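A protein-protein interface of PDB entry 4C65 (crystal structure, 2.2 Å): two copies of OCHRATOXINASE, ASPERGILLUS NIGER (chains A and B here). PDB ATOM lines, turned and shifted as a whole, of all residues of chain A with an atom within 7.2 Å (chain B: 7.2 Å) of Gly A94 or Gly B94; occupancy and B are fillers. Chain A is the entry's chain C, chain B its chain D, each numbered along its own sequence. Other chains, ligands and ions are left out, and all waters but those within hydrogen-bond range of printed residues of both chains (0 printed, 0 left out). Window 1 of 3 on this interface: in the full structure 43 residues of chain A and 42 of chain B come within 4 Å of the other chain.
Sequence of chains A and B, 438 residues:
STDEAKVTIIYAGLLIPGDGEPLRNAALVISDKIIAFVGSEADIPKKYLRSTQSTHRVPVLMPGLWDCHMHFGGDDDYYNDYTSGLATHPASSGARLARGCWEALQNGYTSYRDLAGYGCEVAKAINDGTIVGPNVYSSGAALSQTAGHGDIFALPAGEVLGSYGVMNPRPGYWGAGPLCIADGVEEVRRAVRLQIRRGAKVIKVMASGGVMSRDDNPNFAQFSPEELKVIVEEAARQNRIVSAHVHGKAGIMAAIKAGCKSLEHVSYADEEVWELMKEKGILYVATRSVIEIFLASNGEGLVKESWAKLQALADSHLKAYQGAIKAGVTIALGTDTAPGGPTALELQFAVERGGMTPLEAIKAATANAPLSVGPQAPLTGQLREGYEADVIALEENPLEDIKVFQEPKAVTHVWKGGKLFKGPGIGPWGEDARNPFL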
ATOM      1  N   PHE A  72      23.271 -21.336 -11.345  1.00  0.00           N
ATOM      2  CA  PHE A  72      23.868 -20.858 -10.128  1.00  0.00           C
ATOM      3  C   PHE A  72      23.396 -21.701  -8.967  1.00  0.00           C
ATOM      4  O   PHE A  72      22.582 -21.255  -8.149  1.00  0.00           O
ATOM      5  CB  PHE A  72      23.520 -19.374  -9.930  1.00  0.00           C
ATOM      6  CG  PHE A  72      24.422 -18.427 -10.660  1.00  0.00           C
ATOM      7  CD1 PHE A  72      24.575 -18.491 -12.031  1.00  0.00           C
ATOM      8  CD2 PHE A  72      25.151 -17.471  -9.954  1.00  0.00           C
ATOM      9  CE1 PHE A  72      25.435 -17.621 -12.693  1.00  0.00           C
ATOM     10  CE2 PHE A  72      26.007 -16.609 -10.613  1.00  0.00           C
ATOM     11  CZ  PHE A  72      26.158 -16.696 -11.985  1.00  0.00           C
ATOM     12  N   GLY A  73      23.898 -22.926  -8.903  1.00  0.00           N
ATOM     13  CA  GLY A  73      23.436 -23.894  -7.932  1.00  0.00           C
ATOM     14  C   GLY A  73      24.244 -23.905  -6.650  1.00  0.00           C
ATOM     15  O   GLY A  73      23.667 -23.835  -5.565  1.00  0.00           O
ATOM     16  N   GLY A  74      25.564 -24.019  -6.785  1.00  0.00           N
ATOM     17  CA  GLY A  74      26.485 -24.118  -5.642  1.00  0.00           C
ATOM     18  C   GLY A  74      26.262 -25.283  -4.698  1.00  0.00           C
ATOM     19  O   GLY A  74      26.587 -25.195  -3.517  1.00  0.00           O
ATOM     20  N   THR A  88      20.789 -28.430  -0.001  1.00  0.00           N
ATOM     21  CA  THR A  88      21.907 -27.505   0.217  1.00  0.00           C
ATOM     22  C   THR A  88      21.415 -26.148   0.728  1.00  0.00           C
ATOM     23  O   THR A  88      20.584 -25.476   0.105  1.00  0.00           O
ATOM     24  CB  THR A  88      22.738 -27.279  -1.065  1.00  0.00           C
ATOM     25  OG1 THR A  88      23.300 -28.527  -1.486  1.00  0.00           O
ATOM     26  CG2 THR A  88      23.852 -26.306  -0.832  1.00  0.00           C
ATOM     27  N   HIS A  89      21.958 -25.748   1.869  1.00  0.00           N
ATOM     28  CA  HIS A  89      21.627 -24.446   2.434  1.00  0.00           C
ATOM     29  C   HIS A  89      22.144 -23.349   1.478  1.00  0.00           C
ATOM     30  O   HIS A  89      23.278 -23.403   1.057  1.00  0.00           O
ATOM     31  CB  HIS A  89      22.239 -24.313   3.820  1.00  0.00           C
ATOM     32  CG  HIS A  89      21.677 -23.185   4.601  1.00  0.00           C
ATOM     33  ND1 HIS A  89      22.015 -21.884   4.341  1.00  0.00           N
ATOM     34  CD2 HIS A  89      20.772 -23.148   5.604  1.00  0.00           C
ATOM     35  CE1 HIS A  89      21.362 -21.087   5.159  1.00  0.00           C
ATOM     36  NE2 HIS A  89      20.589 -21.829   5.929  1.00  0.00           N
ATOM     37  N   PRO A  90      21.299 -22.370   1.124  1.00  0.00           N
ATOM     38  CA  PRO A  90      21.781 -21.369   0.169  1.00  0.00           C
ATOM     39  C   PRO A  90      23.034 -20.564   0.577  1.00  0.00           C
ATOM     40  O   PRO A  90      23.720 -20.065  -0.305  1.00  0.00           O
ATOM     41  CB  PRO A  90      20.577 -20.443  -0.030  1.00  0.00           C
ATOM     42  CG  PRO A  90      19.402 -21.226   0.461  1.00  0.00           C
ATOM     43  CD  PRO A  90      19.937 -22.071   1.580  1.00  0.00           C
ATOM     44  N   ALA A  91      23.337 -20.453   1.870  1.00  0.00           N
ATOM     45  CA  ALA A  91      24.594 -19.851   2.301  1.00  0.00           C
ATOM     46  C   ALA A  91      25.814 -20.637   1.826  1.00  0.00           C
ATOM     47  O   ALA A  91      26.793 -20.050   1.408  1.00  0.00           O
ATOM     48  CB  ALA A  91      24.622 -19.683   3.802  1.00  0.00           C
ATOM     49  N   SER A  92      25.750 -21.970   1.892  1.00  0.00           N
ATOM     50  CA  SER A  92      26.759 -22.825   1.301  1.00  0.00           C
ATOM     51  C   SER A  92      26.844 -22.530  -0.189  1.00  0.00           C
ATOM     52  O   SER A  92      27.938 -22.362  -0.729  1.00  0.00           O
ATOM     53  CB  SER A  92      26.432 -24.306   1.509  1.00  0.00           C
ATOM     54  OG  SER A  92      26.297 -24.612   2.881  1.00  0.00           O
ATOM     55  N   SER A  93      25.698 -22.504  -0.860  1.00  0.00           N
ATOM     56  CA  SER A  93      25.665 -22.266  -2.313  1.00  0.00           C
ATOM     57  C   SER A  93      26.337 -20.966  -2.716  1.00  0.00           C
ATOM     58  O   SER A  93      27.174 -20.944  -3.589  1.00  0.00           O
ATOM     59  CB  SER A  93      24.223 -22.238  -2.814  1.00  0.00           C
ATOM     60  OG  SER A  93      23.535 -23.442  -2.496  1.00  0.00           O
ATOM     61  N   GLY A  94      25.964 -19.882  -2.048  1.00  0.00           N
ATOM     62  CA  GLY A  94      26.508 -18.563  -2.341  1.00  0.00           C
ATOM     63  C   GLY A  94      27.998 -18.494  -2.196  1.00  0.00           C
ATOM     64  O   GLY A  94      28.681 -17.911  -3.029  1.00  0.00           O
ATOM     65  N   ALA A  95      28.515 -19.131  -1.147  1.00  0.00           N
ATOM     66  CA  ALA A  95      29.945 -19.180  -0.940  1.00  0.00           C
ATOM     67  C   ALA A  95      30.619 -19.844  -2.137  1.00  0.00           C
ATOM     68  O   ALA A  95      31.592 -19.318  -2.678  1.00  0.00           O
ATOM     69  CB  ALA A  95      30.274 -19.910   0.351  1.00  0.00           C
ATOM     70  N   ARG A  96      30.087 -20.981  -2.565  1.00  0.00           N
ATOM     71  CA  ARG A  96      30.667 -21.715  -3.687  1.00  0.00           C
ATOM     72  C   ARG A  96      30.544 -20.924  -4.982  1.00  0.00           C
ATOM     73  O   ARG A  96      31.467 -20.891  -5.792  1.00  0.00           O
ATOM     74  CB  ARG A  96      30.015 -23.090  -3.855  1.00  0.00           C
ATOM     75  CG  ARG A  96      30.250 -24.023  -2.685  1.00  0.00           C
ATOM     76  CD  ARG A  96      30.122 -25.502  -3.066  1.00  0.00           C
ATOM     77  NE  ARG A  96      30.219 -26.347  -1.888  1.00  0.00           N
ATOM     78  CZ  ARG A  96      29.203 -26.606  -1.073  1.00  0.00           C
ATOM     79  NH1 ARG A  96      27.984 -26.138  -1.309  1.00  0.00           N
ATOM     80  NH2 ARG A  96      29.407 -27.355  -0.004  1.00  0.00           N
ATOM     81  N   LEU A  97      29.407 -20.275  -5.169  1.00  0.00           N
ATOM     82  CA  LEU A  97      29.179 -19.474  -6.371  1.00  0.00           C
ATOM     83  C   LEU A  97      30.118 -18.274  -6.472  1.00  0.00           C
ATOM     84  O   LEU A  97      30.383 -17.777  -7.574  1.00  0.00           O
ATOM     85  CB  LEU A  97      27.713 -19.028  -6.442  1.00  0.00           C
ATOM     86  CG  LEU A  97      26.766 -20.203  -6.709  1.00  0.00           C
ATOM     87  CD1 LEU A  97      25.341 -19.828  -6.349  1.00  0.00           C
ATOM     88  CD2 LEU A  97      26.840 -20.654  -8.169  1.00  0.00           C
ATOM     89  N   ALA A  98      30.635 -17.819  -5.339  1.00  0.00           N
ATOM     90  CA  ALA A  98      31.574 -16.709  -5.325  1.00  0.00           C
ATOM     91  C   ALA A  98      32.882 -17.115  -5.990  1.00  0.00           C
ATOM     92  O   ALA A  98      33.439 -16.353  -6.757  1.00  0.00           O
ATOM     93  CB  ALA A  98      31.820 -16.235  -3.891  1.00  0.00           C
ATOM     94  N   ARG A  99      33.388 -18.300  -5.646  1.00  0.00           N
ATOM     95  CA  ARG A  99      34.553 -18.872  -6.304  1.00  0.00           C
ATOM     96  C   ARG A  99      34.276 -19.025  -7.784  1.00  0.00           C
ATOM     97  O   ARG A  99      35.078 -18.634  -8.609  1.00  0.00           O
ATOM     98  CB  ARG A  99      34.926 -20.238  -5.716  1.00  0.00           C
ATOM     99  CG  ARG A  99      36.105 -20.918  -6.412  1.00  0.00           C
ATOM    100  CD  ARG A  99      37.398 -20.147  -6.139  1.00  0.00           C
ATOM    101  NE  ARG A  99      38.608 -20.774  -6.663  1.00  0.00           N
ATOM    102  CZ  ARG A  99      39.268 -21.776  -6.093  1.00  0.00           C
ATOM    103  NH1 ARG A  99      38.844 -22.323  -4.975  1.00  0.00           N
ATOM    104  NH2 ARG A  99      40.378 -22.232  -6.667  1.00  0.00           N
ATOM    105  N   GLY A 100      33.134 -19.616  -8.107  1.00  0.00           N
ATOM    106  CA  GLY A 100      32.725 -19.836  -9.500  1.00  0.00           C
ATOM    107  C   GLY A 100      32.720 -18.575 -10.321  1.00  0.00           C
ATOM    108  O   GLY A 100      33.267 -18.542 -11.410  1.00  0.00           O
ATOM    109  N   TYR A 118      20.579 -19.169  -7.998  1.00  0.00           N
ATOM    110  CA  TYR A 118      20.654 -18.034  -7.127  1.00  0.00           C
ATOM    111  C   TYR A 118      21.400 -16.852  -7.761  1.00  0.00           C
ATOM    112  O   TYR A 118      21.975 -16.037  -7.055  1.00  0.00           O
ATOM    113  CB  TYR A 118      21.353 -18.461  -5.832  1.00  0.00           C
ATOM    114  CG  TYR A 118      20.652 -19.545  -5.091  1.00  0.00           C
ATOM    115  CD1 TYR A 118      19.399 -19.333  -4.536  1.00  0.00           C
ATOM    116  CD2 TYR A 118      21.240 -20.775  -4.901  1.00  0.00           C
ATOM    117  CE1 TYR A 118      18.744 -20.324  -3.818  1.00  0.00           C
ATOM    118  CE2 TYR A 118      20.593 -21.779  -4.196  1.00  0.00           C
ATOM    119  CZ  TYR A 118      19.341 -21.543  -3.649  1.00  0.00           C
ATOM    120  OH  TYR A 118      18.707 -22.544  -2.953  1.00  0.00           O
ATOM    121  N   VAL A 122      23.099 -13.744  -5.816  1.00  0.00           N
ATOM    122  CA  VAL A 122      24.530 -13.592  -5.881  1.00  0.00           C
ATOM    123  C   VAL A 122      24.929 -12.300  -6.604  1.00  0.00           C
ATOM    124  O   VAL A 122      25.899 -11.651  -6.212  1.00  0.00           O
ATOM    125  CB  VAL A 122      25.183 -14.848  -6.529  1.00  0.00           C
ATOM    126  CG1 VAL A 122      26.657 -14.616  -6.788  1.00  0.00           C
ATOM    127  CG2 VAL A 122      24.992 -16.078  -5.648  1.00  0.00           C
ATOM    128  N   ALA A 125      25.815  -9.400  -4.536  1.00  0.00           N
ATOM    129  CA  ALA A 125      27.132  -9.347  -3.922  1.00  0.00           C
ATOM    130  C   ALA A 125      28.198  -8.939  -4.948  1.00  0.00           C
ATOM    131  O   ALA A 125      29.258  -8.452  -4.575  1.00  0.00           O
ATOM    132  CB  ALA A 125      27.471 -10.686  -3.316  1.00  0.00           C
ATOM    133  N   ILE A 131      32.065  -9.173  -3.932  1.00  0.00           N
ATOM    134  CA  ILE A 131      32.777 -10.147  -4.728  1.00  0.00           C
ATOM    135  C   ILE A 131      32.839  -9.666  -6.180  1.00  0.00           C
ATOM    136  O   ILE A 131      32.327  -8.590  -6.500  1.00  0.00           O
ATOM    137  CB  ILE A 131      32.138 -11.561  -4.659  1.00  0.00           C
ATOM    138  CG1 ILE A 131      30.728 -11.553  -5.209  1.00  0.00           C
ATOM    139  CG2 ILE A 131      32.146 -12.101  -3.239  1.00  0.00           C
ATOM    140  CD1 ILE A 131      30.231 -12.932  -5.552  1.00  0.00           C
ATOM    141  N   PHE B  72      28.877 -14.456  11.141  1.00  0.00           N
ATOM    142  CA  PHE B  72      28.857 -14.799   9.737  1.00  0.00           C
ATOM    143  C   PHE B  72      27.511 -14.406   9.169  1.00  0.00           C
ATOM    144  O   PHE B  72      26.676 -15.246   8.866  1.00  0.00           O
ATOM    145  CB  PHE B  72      29.120 -16.293   9.539  1.00  0.00           C
ATOM    146  CG  PHE B  72      30.585 -16.649   9.482  1.00  0.00           C
ATOM    147  CD1 PHE B  72      31.428 -16.361  10.541  1.00  0.00           C
ATOM    148  CD2 PHE B  72      31.111 -17.299   8.372  1.00  0.00           C
ATOM    149  CE1 PHE B  72      32.765 -16.721  10.494  1.00  0.00           C
ATOM    150  CE2 PHE B  72      32.443 -17.658   8.325  1.00  0.00           C
ATOM    151  CZ  PHE B  72      33.271 -17.371   9.379  1.00  0.00           C
ATOM    152  N   GLY B  73      27.338 -13.103   9.000  1.00  0.00           N
ATOM    153  CA  GLY B  73      26.065 -12.550   8.572  1.00  0.00           C
ATOM    154  C   GLY B  73      25.944 -12.397   7.086  1.00  0.00           C
ATOM    155  O   GLY B  73      24.948 -12.826   6.495  1.00  0.00           O
ATOM    156  N   GLY B  74      26.929 -11.732   6.478  1.00  0.00           N
ATOM    157  CA  GLY B  74      26.901 -11.388   5.038  1.00  0.00           C
ATOM    158  C   GLY B  74      25.719 -10.566   4.549  1.00  0.00           C
ATOM    159  O   GLY B  74      25.340 -10.649   3.374  1.00  0.00           O
ATOM    160  N   THR B  88      17.856 -10.650   4.139  1.00  0.00           N
ATOM    161  CA  THR B  88      18.927 -11.003   3.205  1.00  0.00           C
ATOM    162  C   THR B  88      18.845 -12.485   2.879  1.00  0.00           C
ATOM    163  O   THR B  88      18.877 -13.354   3.764  1.00  0.00           O
ATOM    164  CB  THR B  88      20.328 -10.684   3.774  1.00  0.00           C
ATOM    165  OG1 THR B  88      20.464  -9.281   3.978  1.00  0.00           O
ATOM    166  CG2 THR B  88      21.420 -11.129   2.823  1.00  0.00           C
ATOM    167  N   HIS B  89      18.761 -12.774   1.590  1.00  0.00           N
ATOM    168  CA  HIS B  89      18.770 -14.153   1.146  1.00  0.00           C
ATOM    169  C   HIS B  89      20.118 -14.806   1.474  1.00  0.00           C
ATOM    170  O   HIS B  89      21.149 -14.230   1.212  1.00  0.00           O
ATOM    171  CB  HIS B  89      18.479 -14.225  -0.338  1.00  0.00           C
ATOM    172  CG  HIS B  89      18.111 -15.597  -0.800  1.00  0.00           C
ATOM    173  ND1 HIS B  89      19.046 -16.582  -0.977  1.00  0.00           N
ATOM    174  CD2 HIS B  89      16.922 -16.143  -1.133  1.00  0.00           C
ATOM    175  CE1 HIS B  89      18.456 -17.676  -1.421  1.00  0.00           C
ATOM    176  NE2 HIS B  89      17.164 -17.434  -1.519  1.00  0.00           N
ATOM    177  N   PRO B  90      20.118 -16.018   2.037  1.00  0.00           N
ATOM    178  CA  PRO B  90      21.406 -16.553   2.479  1.00  0.00           C
ATOM    179  C   PRO B  90      22.420 -16.820   1.359  1.00  0.00           C
ATOM    180  O   PRO B  90      23.613 -16.884   1.639  1.00  0.00           O
ATOM    181  CB  PRO B  90      21.028 -17.863   3.185  1.00  0.00           C
ATOM    182  CG  PRO B  90      19.581 -17.735   3.529  1.00  0.00           C
ATOM    183  CD  PRO B  90      19.001 -16.903   2.416  1.00  0.00           C
ATOM    184  N   ALA B  91      21.965 -16.971   0.113  1.00  0.00           N
ATOM    185  CA  ALA B  91      22.875 -17.040  -1.042  1.00  0.00           C
ATOM    186  C   ALA B  91      23.680 -15.768  -1.236  1.00  0.00           C
ATOM    187  O   ALA B  91      24.874 -15.836  -1.489  1.00  0.00           O
ATOM    188  CB  ALA B  91      22.125 -17.385  -2.307  1.00  0.00           C
ATOM    189  N   SER B  92      23.045 -14.606  -1.080  1.00  0.00           N
ATOM    190  CA  SER B  92      23.759 -13.332  -1.020  1.00  0.00           C
ATOM    191  C   SER B  92      24.772 -13.351   0.126  1.00  0.00           C
ATOM    192  O   SER B  92      25.934 -12.997  -0.053  1.00  0.00           O
ATOM    193  CB  SER B  92      22.797 -12.166  -0.800  1.00  0.00           C
ATOM    194  OG  SER B  92      21.812 -12.122  -1.791  1.00  0.00           O
ATOM    195  N   SER B  93      24.332 -13.781   1.304  1.00  0.00           N
ATOM    196  CA  SER B  93      25.210 -13.834   2.504  1.00  0.00           C
ATOM    197  C   SER B  93      26.453 -14.676   2.292  1.00  0.00           C
ATOM    198  O   SER B  93      27.563 -14.221   2.528  1.00  0.00           O
ATOM    199  CB  SER B  93      24.457 -14.389   3.718  1.00  0.00           C
ATOM    200  OG  SER B  93      23.301 -13.629   3.991  1.00  0.00           O
ATOM    201  N   GLY B  94      26.256 -15.900   1.809  1.00  0.00           N
ATOM    202  CA  GLY B  94      27.360 -16.802   1.565  1.00  0.00           C
ATOM    203  C   GLY B  94      28.396 -16.227   0.612  1.00  0.00           C
ATOM    204  O   GLY B  94      29.598 -16.390   0.823  1.00  0.00           O
ATOM    205  N   ALA B  95      27.929 -15.594  -0.457  1.00  0.00           N
ATOM    206  CA  ALA B  95      28.820 -15.017  -1.415  1.00  0.00           C
ATOM    207  C   ALA B  95      29.695 -13.989  -0.708  1.00  0.00           C
ATOM    208  O   ALA B  95      30.913 -13.963  -0.902  1.00  0.00           O
ATOM    209  CB  ALA B  95      28.030 -14.379  -2.560  1.00  0.00           C
ATOM    210  N   ARG B  96      29.071 -13.132   0.093  1.00  0.00           N
ATOM    211  CA  ARG B  96      29.813 -12.069   0.777  1.00  0.00           C
ATOM    212  C   ARG B  96      30.781 -12.643   1.809  1.00  0.00           C
ATOM    213  O   ARG B  96      31.913 -12.183   1.939  1.00  0.00           O
ATOM    214  CB  ARG B  96      28.862 -11.061   1.459  1.00  0.00           C
ATOM    215  CG  ARG B  96      27.995 -10.275   0.493  1.00  0.00           C
ATOM    216  CD  ARG B  96      27.495  -8.958   1.082  1.00  0.00           C
ATOM    217  NE  ARG B  96      26.565  -8.313   0.170  1.00  0.00           N
ATOM    218  CZ  ARG B  96      25.260  -8.558   0.073  1.00  0.00           C
ATOM    219  NH1 ARG B  96      24.604  -9.446   0.816  1.00  0.00           N
ATOM    220  NH2 ARG B  96      24.596  -7.905  -0.873  1.00  0.00           N
ATOM    221  N   LEU B  97      30.333 -13.669   2.517  1.00  0.00           N
ATOM    222  CA  LEU B  97      31.176 -14.328   3.502  1.00  0.00           C
ATOM    223  C   LEU B  97      32.419 -14.995   2.885  1.00  0.00           C
ATOM    224  O   LEU B  97      33.414 -15.207   3.572  1.00  0.00           O
ATOM    225  CB  LEU B  97      30.349 -15.335   4.308  1.00  0.00           C
ATOM    226  CG  LEU B  97      29.329 -14.643   5.213  1.00  0.00           C
ATOM    227  CD1 LEU B  97      28.248 -15.619   5.658  1.00  0.00           C
ATOM    228  CD2 LEU B  97      30.006 -14.016   6.427  1.00  0.00           C
ATOM    229  N   ALA B  98      32.343 -15.342   1.599  1.00  0.00           N
ATOM    230  CA  ALA B  98      33.452 -15.965   0.895  1.00  0.00           C
ATOM    231  C   ALA B  98      34.590 -14.975   0.727  1.00  0.00           C
ATOM    232  O   ALA B  98      35.741 -15.329   0.996  1.00  0.00           O
ATOM    233  CB  ALA B  98      33.023 -16.491  -0.462  1.00  0.00           C
ATOM    234  N   ARG B  99      34.262 -13.739   0.351  1.00  0.00           N
ATOM    235  CA  ARG B  99      35.248 -12.652   0.349  1.00  0.00           C
ATOM    236  C   ARG B  99      35.821 -12.429   1.750  1.00  0.00           C
ATOM    237  O   ARG B  99      37.024 -12.364   1.927  1.00  0.00           O
ATOM    238  CB  ARG B  99      34.636 -11.362  -0.153  1.00  0.00           C
ATOM    239  CG  ARG B  99      35.586 -10.175  -0.140  1.00  0.00           C
ATOM    240  CD  ARG B  99      36.691 -10.362  -1.166  1.00  0.00           C
ATOM    241  NE  ARG B  99      37.569  -9.203  -1.280  1.00  0.00           N
ATOM    242  CZ  ARG B  99      37.308  -8.129  -2.026  1.00  0.00           C
ATOM    243  NH1 ARG B  99      36.168  -8.018  -2.704  1.00  0.00           N
ATOM    244  NH2 ARG B  99      38.186  -7.130  -2.066  1.00  0.00           N
ATOM    245  N   GLY B 100      34.942 -12.332   2.740  1.00  0.00           N
ATOM    246  CA  GLY B 100      35.340 -12.124   4.115  1.00  0.00           C
ATOM    247  C   GLY B 100      36.328 -13.158   4.599  1.00  0.00           C
ATOM    248  O   GLY B 100      37.322 -12.834   5.214  1.00  0.00           O
ATOM    249  N   TYR B 118      26.030 -17.981   9.571  1.00  0.00           N
ATOM    250  CA  TYR B 118      26.049 -19.086   8.649  1.00  0.00           C
ATOM    251  C   TYR B 118      27.420 -19.754   8.589  1.00  0.00           C
ATOM    252  O   TYR B 118      27.777 -20.339   7.576  1.00  0.00           O
ATOM    253  CB  TYR B 118      25.648 -18.578   7.264  1.00  0.00           C
ATOM    254  CG  TYR B 118      24.266 -17.988   7.193  1.00  0.00           C
ATOM    255  CD1 TYR B 118      23.149 -18.770   7.420  1.00  0.00           C
ATOM    256  CD2 TYR B 118      24.076 -16.670   6.869  1.00  0.00           C
ATOM    257  CE1 TYR B 118      21.881 -18.244   7.347  1.00  0.00           C
ATOM    258  CE2 TYR B 118      22.810 -16.126   6.786  1.00  0.00           C
ATOM    259  CZ  TYR B 118      21.714 -16.914   7.029  1.00  0.00           C
ATOM    260  OH  TYR B 118      20.441 -16.377   6.930  1.00  0.00           O
ATOM    261  N   VAL B 122      28.826 -22.078   5.619  1.00  0.00           N
ATOM    262  CA  VAL B 122      29.969 -21.605   4.858  1.00  0.00           C
ATOM    263  C   VAL B 122      31.211 -22.501   5.063  1.00  0.00           C
ATOM    264  O   VAL B 122      31.938 -22.765   4.101  1.00  0.00           O
ATOM    265  CB  VAL B 122      30.289 -20.145   5.206  1.00  0.00           C
ATOM    266  CG1 VAL B 122      31.593 -19.708   4.568  1.00  0.00           C
ATOM    267  CG2 VAL B 122      29.150 -19.237   4.747  1.00  0.00           C
ATOM    268  N   ALA B 125      31.885 -25.042   2.464  1.00  0.00           N
ATOM    269  CA  ALA B 125      32.507 -24.616   1.224  1.00  0.00           C
ATOM    270  C   ALA B 125      34.003 -24.413   1.402  1.00  0.00           C
ATOM    271  O   ALA B 125      34.761 -24.467   0.450  1.00  0.00           O
ATOM    272  CB  ALA B 125      31.849 -23.356   0.717  1.00  0.00           C
ATOM    273  N   ILE B 131      36.155 -22.744  -1.532  1.00  0.00           N
ATOM    274  CA  ILE B 131      36.696 -21.461  -1.148  1.00  0.00           C
ATOM    275  C   ILE B 131      37.739 -21.685  -0.087  1.00  0.00           C
ATOM    276  O   ILE B 131      37.987 -22.815   0.332  1.00  0.00           O
ATOM    277  CB  ILE B 131      35.621 -20.462  -0.660  1.00  0.00           C
ATOM    278  CG1 ILE B 131      34.908 -20.978   0.582  1.00  0.00           C
ATOM    279  CG2 ILE B 131      34.608 -20.155  -1.760  1.00  0.00           C
ATOM    280  CD1 ILE B 131      34.171 -19.893   1.329  1.00  0.00           C
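O of Phe A72 sits at hydrogen-bond distance from N of Tyr A118.
O of Gly A74 is in hydrogen-bond range of NH1 of Arg A96 (2.8 Å).
The backbone NH (N) of Ala A91 lies within hydrogen-bond range of a ring nitrogen (ND1) of His A89 (3.1 Å).
The backbone NH (N) of Ile A131 is in hydrogen-bond range of the backbone carbonyl oxygen (O) of Ala A125.
The backbone carbonyl oxygen (O) of Phe B72 lies within hydrogen-bond range of the backbone NH (N) of Tyr B118.
O of Gly B74 lies within hydrogen-bond range of NH1 of Arg B96 (2.9 Å).
His A89 touches Pro B90 (CE1 to CB, 3.8 Å).
Ala B91 touches Pro A90 (CA to O, 3.2 Å).
Pro B90 touches Ala A91.
Ala B98 touches Ala A95.
CB of Ala B125 touches CB of Ala A95, at 3.8 Å.
Ile B131 touches Ala A95 (CG2 to O, 3.3 Å).
Ala A98 touches Ala B95 (CB to O, 3.9 Å).
His B89 touches Tyr A118 (CE1 to CE1, 3.6 Å).
Tyr A118 touches Ala B91 (CB to CB, 3.8 Å).
O of Ala B95 touches CG2 of Ile A131, 3.2 Å away.
Phe A72 touches none of the printed residues of chain B.
Thr A88 touches none of the printed residues of chain B.
Printed residues of chain B within 4 Å of Tyr A118: His B89 (3.6 Å) and Ala B91 (3.8 Å).
Of the printed residues of chain A, Pro B90 touches His A89, Pro A90 and Ala A91.
Gly B94 touches just these residues of chain A: Ala A91, Gly A94 and Ala A95.
The nearest printed residue of chain A that does not touch Gly B94 is Ala A98 (5.2 Å).
Of the 20 printed residues of chain B, 10 touch a printed residue of chain A.
Hydrophobic or aromatic side chains of chain A that line the printed part of chain B: His A89, Pro A90, Ala A91, Ala A95, Ala A98, Tyr A118, Ala A125 and Ile A131.
Among the printed residues, 25 pairs touch across the chains.
Among the printed residues, no Asp or Glu carboxylate lies within 4 Å of a Lys or Arg side-chain nitrogen of the other chain.
His A89 touches Pro B90, and with the chains exchanged Pro A90 touches His B89.
His A89 touches Tyr B118, and with the chains exchanged Tyr A118 touches His B89.
Ala A95 touches Ile B131, and with the chains exchanged Ile A131 touches Ala B95.
Arg A96 touches Ala B125, and with the chains exchanged Ala A125 touches Arg B96.
Of the 25 pairs that touch across the chains among the printed residues, 24 have their exchanged pair printed and touching as well.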
